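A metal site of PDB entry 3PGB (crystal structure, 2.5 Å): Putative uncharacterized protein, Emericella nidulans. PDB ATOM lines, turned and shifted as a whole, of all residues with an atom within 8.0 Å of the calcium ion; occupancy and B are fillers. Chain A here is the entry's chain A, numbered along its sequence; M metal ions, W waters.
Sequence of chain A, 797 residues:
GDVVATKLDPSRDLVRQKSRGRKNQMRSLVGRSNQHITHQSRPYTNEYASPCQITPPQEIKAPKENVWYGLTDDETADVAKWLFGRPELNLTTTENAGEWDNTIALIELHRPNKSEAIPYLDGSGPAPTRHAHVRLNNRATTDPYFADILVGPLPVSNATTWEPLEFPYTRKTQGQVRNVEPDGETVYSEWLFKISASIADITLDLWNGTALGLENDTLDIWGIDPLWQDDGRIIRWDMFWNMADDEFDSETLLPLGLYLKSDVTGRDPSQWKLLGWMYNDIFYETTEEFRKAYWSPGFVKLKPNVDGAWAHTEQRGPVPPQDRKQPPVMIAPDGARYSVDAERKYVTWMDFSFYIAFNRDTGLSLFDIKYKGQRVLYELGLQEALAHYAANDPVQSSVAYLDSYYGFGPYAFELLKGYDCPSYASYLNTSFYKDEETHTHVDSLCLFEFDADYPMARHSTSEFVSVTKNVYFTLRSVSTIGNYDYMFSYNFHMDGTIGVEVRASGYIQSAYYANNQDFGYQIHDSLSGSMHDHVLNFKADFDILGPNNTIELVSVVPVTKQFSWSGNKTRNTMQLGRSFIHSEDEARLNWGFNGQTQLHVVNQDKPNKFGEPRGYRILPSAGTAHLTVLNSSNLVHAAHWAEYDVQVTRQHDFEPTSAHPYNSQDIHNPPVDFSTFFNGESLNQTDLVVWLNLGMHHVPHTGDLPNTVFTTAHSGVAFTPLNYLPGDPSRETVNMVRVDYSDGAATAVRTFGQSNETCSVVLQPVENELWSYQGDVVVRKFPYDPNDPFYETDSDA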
ATOM      1  N   GLU A 584      15.544 -22.864  -0.363  1.00  0.00           N
ATOM      2  CA  GLU A 584      15.841 -22.601  -1.761  1.00  0.00           C
ATOM      3  C   GLU A 584      17.336 -22.652  -2.102  1.00  0.00           C
ATOM      4  O   GLU A 584      17.699 -22.701  -3.281  1.00  0.00           O
ATOM      5  CB  GLU A 584      15.290 -21.224  -2.155  1.00  0.00           C
ATOM      6  CG  GLU A 584      13.770 -21.174  -2.248  1.00  0.00           C
ATOM      7  CD  GLU A 584      13.246 -19.803  -2.644  1.00  0.00           C
ATOM      8  OE1 GLU A 584      13.966 -18.802  -2.453  1.00  0.00           O
ATOM      9  OE2 GLU A 584      12.100 -19.729  -3.145  1.00  0.00           O
ATOM     10  N   VAL A 648      12.920 -26.052  -7.240  1.00  0.00           N
ATOM     11  CA  VAL A 648      11.811 -25.762  -6.350  1.00  0.00           C
ATOM     12  C   VAL A 648      11.989 -24.392  -5.716  1.00  0.00           C
ATOM     13  O   VAL A 648      13.061 -24.068  -5.205  1.00  0.00           O
ATOM     14  CB  VAL A 648      11.680 -26.840  -5.259  1.00  0.00           C
ATOM     15  CG1 VAL A 648      10.397 -26.630  -4.482  1.00  0.00           C
ATOM     16  CG2 VAL A 648      11.694 -28.236  -5.889  1.00  0.00           C
ATOM     17  N   THR A 649      10.937 -23.583  -5.783  1.00  0.00           N
ATOM     18  CA  THR A 649      10.917 -22.248  -5.197  1.00  0.00           C
ATOM     19  C   THR A 649       9.633 -22.068  -4.424  1.00  0.00           C
ATOM     20  O   THR A 649       8.647 -22.771  -4.650  1.00  0.00           O
ATOM     21  CB  THR A 649      10.956 -21.138  -6.265  1.00  0.00           C
ATOM     22  OG1 THR A 649       9.759 -21.182  -7.045  1.00  0.00           O
ATOM     23  CG2 THR A 649      12.167 -21.280  -7.164  1.00  0.00           C
ATOM     24  N   ARG A 650       9.647 -21.103  -3.505  1.00  0.00           N
ATOM     25  CA  ARG A 650       8.450 -20.774  -2.756  1.00  0.00           C
ATOM     26  C   ARG A 650       7.518 -19.986  -3.649  1.00  0.00           C
ATOM     27  O   ARG A 650       7.963 -19.133  -4.417  1.00  0.00           O
ATOM     28  CB  ARG A 650       8.780 -19.975  -1.506  1.00  0.00           C
ATOM     29  CG  ARG A 650       7.564 -19.710  -0.664  1.00  0.00           C
ATOM     30  CD  ARG A 650       7.917 -19.191   0.694  1.00  0.00           C
ATOM     31  NE  ARG A 650       6.748 -19.147   1.545  1.00  0.00           N
ATOM     32  CZ  ARG A 650       6.727 -18.610   2.761  1.00  0.00           C
ATOM     33  NH1 ARG A 650       7.834 -18.070   3.287  1.00  0.00           N
ATOM     34  NH2 ARG A 650       5.592 -18.624   3.469  1.00  0.00           N
ATOM     35  N   GLN A 651       6.218 -20.292  -3.547  1.00  0.00           N
ATOM     36  CA  GLN A 651       5.214 -19.642  -4.384  1.00  0.00           C
ATOM     37  C   GLN A 651       5.071 -18.158  -4.020  1.00  0.00           C
ATOM     38  O   GLN A 651       5.053 -17.791  -2.850  1.00  0.00           O
ATOM     39  CB  GLN A 651       3.859 -20.353  -4.245  1.00  0.00           C
ATOM     40  CG  GLN A 651       2.839 -20.032  -5.357  1.00  0.00           C
ATOM     41  CD  GLN A 651       2.114 -18.694  -5.182  1.00  0.00           C
ATOM     42  OE1 GLN A 651       2.003 -18.170  -4.076  1.00  0.00           O
ATOM     43  NE2 GLN A 651       1.614 -18.151  -6.293  1.00  0.00           N
ATOM     44  N   HIS A 652       4.983 -17.335  -5.047  1.00  0.00           N
ATOM     45  CA  HIS A 652       4.630 -15.935  -4.902  1.00  0.00           C
ATOM     46  C   HIS A 652       3.751 -15.552  -6.071  1.00  0.00           C
ATOM     47  O   HIS A 652       3.915 -16.076  -7.167  1.00  0.00           O
ATOM     48  CB  HIS A 652       5.882 -15.061  -4.894  1.00  0.00           C
ATOM     49  CG  HIS A 652       6.775 -15.307  -3.716  1.00  0.00           C
ATOM     50  ND1 HIS A 652       6.347 -15.145  -2.411  1.00  0.00           N
ATOM     51  CD2 HIS A 652       8.067 -15.694  -3.647  1.00  0.00           C
ATOM     52  CE1 HIS A 652       7.339 -15.431  -1.594  1.00  0.00           C
ATOM     53  NE2 HIS A 652       8.397 -15.771  -2.318  1.00  0.00           N
ATOM     54  N   PHE A 654       3.901 -12.668  -7.341  1.00  0.00           N
ATOM     55  CA  PHE A 654       4.823 -11.877  -8.160  1.00  0.00           C
ATOM     56  C   PHE A 654       5.871 -12.735  -8.912  1.00  0.00           C
ATOM     57  O   PHE A 654       6.776 -12.192  -9.542  1.00  0.00           O
ATOM     58  CB  PHE A 654       5.501 -10.774  -7.331  1.00  0.00           C
ATOM     59  CG  PHE A 654       6.140 -11.255  -6.056  1.00  0.00           C
ATOM     60  CD1 PHE A 654       7.437 -11.759  -6.064  1.00  0.00           C
ATOM     61  CD2 PHE A 654       5.474 -11.147  -4.845  1.00  0.00           C
ATOM     62  CE1 PHE A 654       8.033 -12.186  -4.891  1.00  0.00           C
ATOM     63  CE2 PHE A 654       6.049 -11.580  -3.650  1.00  0.00           C
ATOM     64  CZ  PHE A 654       7.342 -12.092  -3.669  1.00  0.00           C
ATOM     65  N   GLU A 655       5.730 -14.070  -8.847  1.00  0.00           N
ATOM     66  CA  GLU A 655       6.529 -14.970  -9.680  1.00  0.00           C
ATOM     67  C   GLU A 655       5.612 -15.993 -10.346  1.00  0.00           C
ATOM     68  O   GLU A 655       5.702 -17.194 -10.061  1.00  0.00           O
ATOM     69  CB  GLU A 655       7.587 -15.700  -8.836  1.00  0.00           C
ATOM     70  CG  GLU A 655       8.713 -14.809  -8.293  1.00  0.00           C
ATOM     71  CD  GLU A 655       9.559 -15.473  -7.218  1.00  0.00           C
ATOM     72  OE1 GLU A 655       9.275 -16.642  -6.820  1.00  0.00           O
ATOM     73  OE2 GLU A 655      10.525 -14.827  -6.747  1.00  0.00           O
ATOM     74  N   PHE A 674      15.112 -15.897 -13.925  1.00  0.00           N
ATOM     75  CA  PHE A 674      14.751 -17.019 -13.058  1.00  0.00           C
ATOM     76  C   PHE A 674      15.710 -17.181 -11.875  1.00  0.00           C
ATOM     77  O   PHE A 674      15.273 -17.529 -10.780  1.00  0.00           O
ATOM     78  CB  PHE A 674      14.650 -18.317 -13.874  1.00  0.00           C
ATOM     79  CG  PHE A 674      14.047 -19.472 -13.107  1.00  0.00           C
ATOM     80  CD1 PHE A 674      12.699 -19.475 -12.772  1.00  0.00           C
ATOM     81  CD2 PHE A 674      14.828 -20.549 -12.717  1.00  0.00           C
ATOM     82  CE1 PHE A 674      12.150 -20.534 -12.069  1.00  0.00           C
ATOM     83  CE2 PHE A 674      14.279 -21.608 -12.014  1.00  0.00           C
ATOM     84  CZ  PHE A 674      12.937 -21.608 -11.692  1.00  0.00           C
ATOM     85  N   SER A 675      17.004 -16.906 -12.079  1.00  0.00           N
ATOM     86  CA  SER A 675      18.000 -16.991 -10.986  1.00  0.00           C
ATOM     87  C   SER A 675      17.588 -16.265  -9.708  1.00  0.00           C
ATOM     88  O   SER A 675      17.894 -16.724  -8.610  1.00  0.00           O
ATOM     89  CB  SER A 675      19.363 -16.448 -11.422  1.00  0.00           C
ATOM     90  OG  SER A 675      20.053 -17.416 -12.168  1.00  0.00           O
ATOM     91  N   THR A 676      16.916 -15.127  -9.876  1.00  0.00           N
ATOM     92  CA  THR A 676      16.583 -14.232  -8.773  1.00  0.00           C
ATOM     93  C   THR A 676      15.443 -14.776  -7.901  1.00  0.00           C
ATOM     94  O   THR A 676      15.163 -14.234  -6.837  1.00  0.00           O
ATOM     95  CB  THR A 676      16.208 -12.819  -9.297  1.00  0.00           C
ATOM     96  OG1 THR A 676      14.955 -12.872  -9.987  1.00  0.00           O
ATOM     97  CG2 THR A 676      17.289 -12.271 -10.237  1.00  0.00           C
ATOM     98  N   PHE A 677      14.798 -15.853  -8.344  1.00  0.00           N
ATOM     99  CA  PHE A 677      13.773 -16.547  -7.539  1.00  0.00           C
ATOM    100  C   PHE A 677      14.392 -17.181  -6.295  1.00  0.00           C
ATOM    101  O   PHE A 677      13.685 -17.431  -5.320  1.00  0.00           O
ATOM    102  CB  PHE A 677      13.088 -17.659  -8.349  1.00  0.00           C
ATOM    103  CG  PHE A 677      12.077 -17.174  -9.370  1.00  0.00           C
ATOM    104  CD1 PHE A 677      12.145 -15.884  -9.931  1.00  0.00           C
ATOM    105  CD2 PHE A 677      11.083 -18.042  -9.798  1.00  0.00           C
ATOM    106  CE1 PHE A 677      11.216 -15.485 -10.883  1.00  0.00           C
ATOM    107  CE2 PHE A 677      10.146 -17.645 -10.755  1.00  0.00           C
ATOM    108  CZ  PHE A 677      10.215 -16.355 -11.299  1.00  0.00           C
ATOM    109  N   PHE A 678      15.695 -17.463  -6.349  1.00  0.00           N
ATOM    110  CA  PHE A 678      16.382 -18.203  -5.285  1.00  0.00           C
ATOM    111  C   PHE A 678      17.104 -17.249  -4.328  1.00  0.00           C
ATOM    112  O   PHE A 678      18.234 -16.815  -4.576  1.00  0.00           O
ATOM    113  CB  PHE A 678      17.337 -19.226  -5.907  1.00  0.00           C
ATOM    114  CG  PHE A 678      16.639 -20.195  -6.814  1.00  0.00           C
ATOM    115  CD1 PHE A 678      16.143 -21.402  -6.327  1.00  0.00           C
ATOM    116  CD2 PHE A 678      16.402 -19.872  -8.143  1.00  0.00           C
ATOM    117  CE1 PHE A 678      15.457 -22.279  -7.153  1.00  0.00           C
ATOM    118  CE2 PHE A 678      15.716 -20.741  -8.975  1.00  0.00           C
ATOM    119  CZ  PHE A 678      15.250 -21.954  -8.474  1.00  0.00           C
ATOM    120  N   ASN A 679      16.408 -16.936  -3.238  1.00  0.00           N
ATOM    121  CA  ASN A 679      16.866 -16.020  -2.203  1.00  0.00           C
ATOM    122  C   ASN A 679      16.656 -16.626  -0.824  1.00  0.00           C
ATOM    123  O   ASN A 679      16.133 -15.978   0.088  1.00  0.00           O
ATOM    124  CB  ASN A 679      16.152 -14.666  -2.322  1.00  0.00           C
ATOM    125  CG  ASN A 679      14.640 -14.782  -2.187  1.00  0.00           C
ATOM    126  OD1 ASN A 679      14.063 -15.846  -2.460  1.00  0.00           O
ATOM    127  ND2 ASN A 679      13.983 -13.704  -1.760  1.00  0.00           N
ATOM    128  N   GLY A 680      17.050 -17.888  -0.683  1.00  0.00           N
ATOM    129  CA  GLY A 680      17.136 -18.564   0.618  1.00  0.00           C
ATOM    130  C   GLY A 680      15.855 -18.736   1.423  1.00  0.00           C
ATOM    131  O   GLY A 680      15.923 -18.969   2.625  1.00  0.00           O
ATOM    132  N   GLU A 681      14.706 -18.657   0.770  1.00  0.00           N
ATOM    133  CA  GLU A 681      13.422 -18.838   1.454  1.00  0.00           C
ATOM    134  C   GLU A 681      13.206 -20.288   1.855  1.00  0.00           C
ATOM    135  O   GLU A 681      13.680 -21.214   1.184  1.00  0.00           O
ATOM    136  CB  GLU A 681      12.266 -18.386   0.571  1.00  0.00           C
ATOM    137  CG  GLU A 681      12.228 -16.897   0.296  1.00  0.00           C
ATOM    138  CD  GLU A 681      10.971 -16.481  -0.444  1.00  0.00           C
ATOM    139  OE1 GLU A 681      10.908 -16.674  -1.669  1.00  0.00           O
ATOM    140  OE2 GLU A 681      10.054 -15.961   0.224  1.00  0.00           O
ATOM    141  N   SER A 682      12.474 -20.493   2.943  1.00  0.00           N
ATOM    142  CA  SER A 682      12.232 -21.818   3.476  1.00  0.00           C
ATOM    143  C   SER A 682      11.213 -22.570   2.615  1.00  0.00           C
ATOM    144  O   SER A 682      10.201 -22.009   2.192  1.00  0.00           O
ATOM    145  CB  SER A 682      11.719 -21.738   4.919  1.00  0.00           C
ATOM    146  OG  SER A 682      11.432 -23.032   5.434  1.00  0.00           O
ATOM    147  N   LEU A 683      11.497 -23.850   2.381  1.00  0.00           N
ATOM    148  CA  LEU A 683      10.589 -24.732   1.668  1.00  0.00           C
ATOM    149  C   LEU A 683      10.125 -25.854   2.596  1.00  0.00           C
ATOM    150  O   LEU A 683       9.660 -26.901   2.127  1.00  0.00           O
ATOM    151  CB  LEU A 683      11.281 -25.296   0.414  1.00  0.00           C
ATOM    152  CG  LEU A 683      11.811 -24.274  -0.606  1.00  0.00           C
ATOM    153  CD1 LEU A 683      12.631 -24.977  -1.672  1.00  0.00           C
ATOM    154  CD2 LEU A 683      10.678 -23.475  -1.239  1.00  0.00           C
HETATM  155 CA    CA M   1      12.389 -17.154  -3.435  1.00  0.00          CA
HETATM  156  O   HOH W   1      11.768 -15.056  -4.328  1.00  0.00           O
HETATM  157  O   HOH W   2      10.420 -17.746  -4.752  1.00  0.00           O
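The calcium ion is bound by the backbone carbonyl oxygen (O) of Phe 677 (2.3 Å), the side-chain amide oxygen (OD1) of Asn 679 (2.3 Å), the side-chain carboxylate (OE1) of Glu 681 (2.4 Å), water W1 (2.4 Å), water W2 (2.4 Å), the side-chain carboxylate (OE1) of Glu 584 (2.5 Å) and the side-chain carboxylate (OE2) of Glu 584 (2.6 Å). The calcium ion has seven donor atoms within binding distance.
OE2 of Glu 681 lies within hydrogen-bond range of NE2 of His 652 (3.0 Å). OE2 of Glu 584 lies close to N of Arg 650, 2.8 Å away.
Water W2 bridges the side-chain carboxylate of Glu 655 and the backbone carbonyl oxygen of Arg 650.
Of the 18 residues printed, 4 come within 4 Å of the calcium ion.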
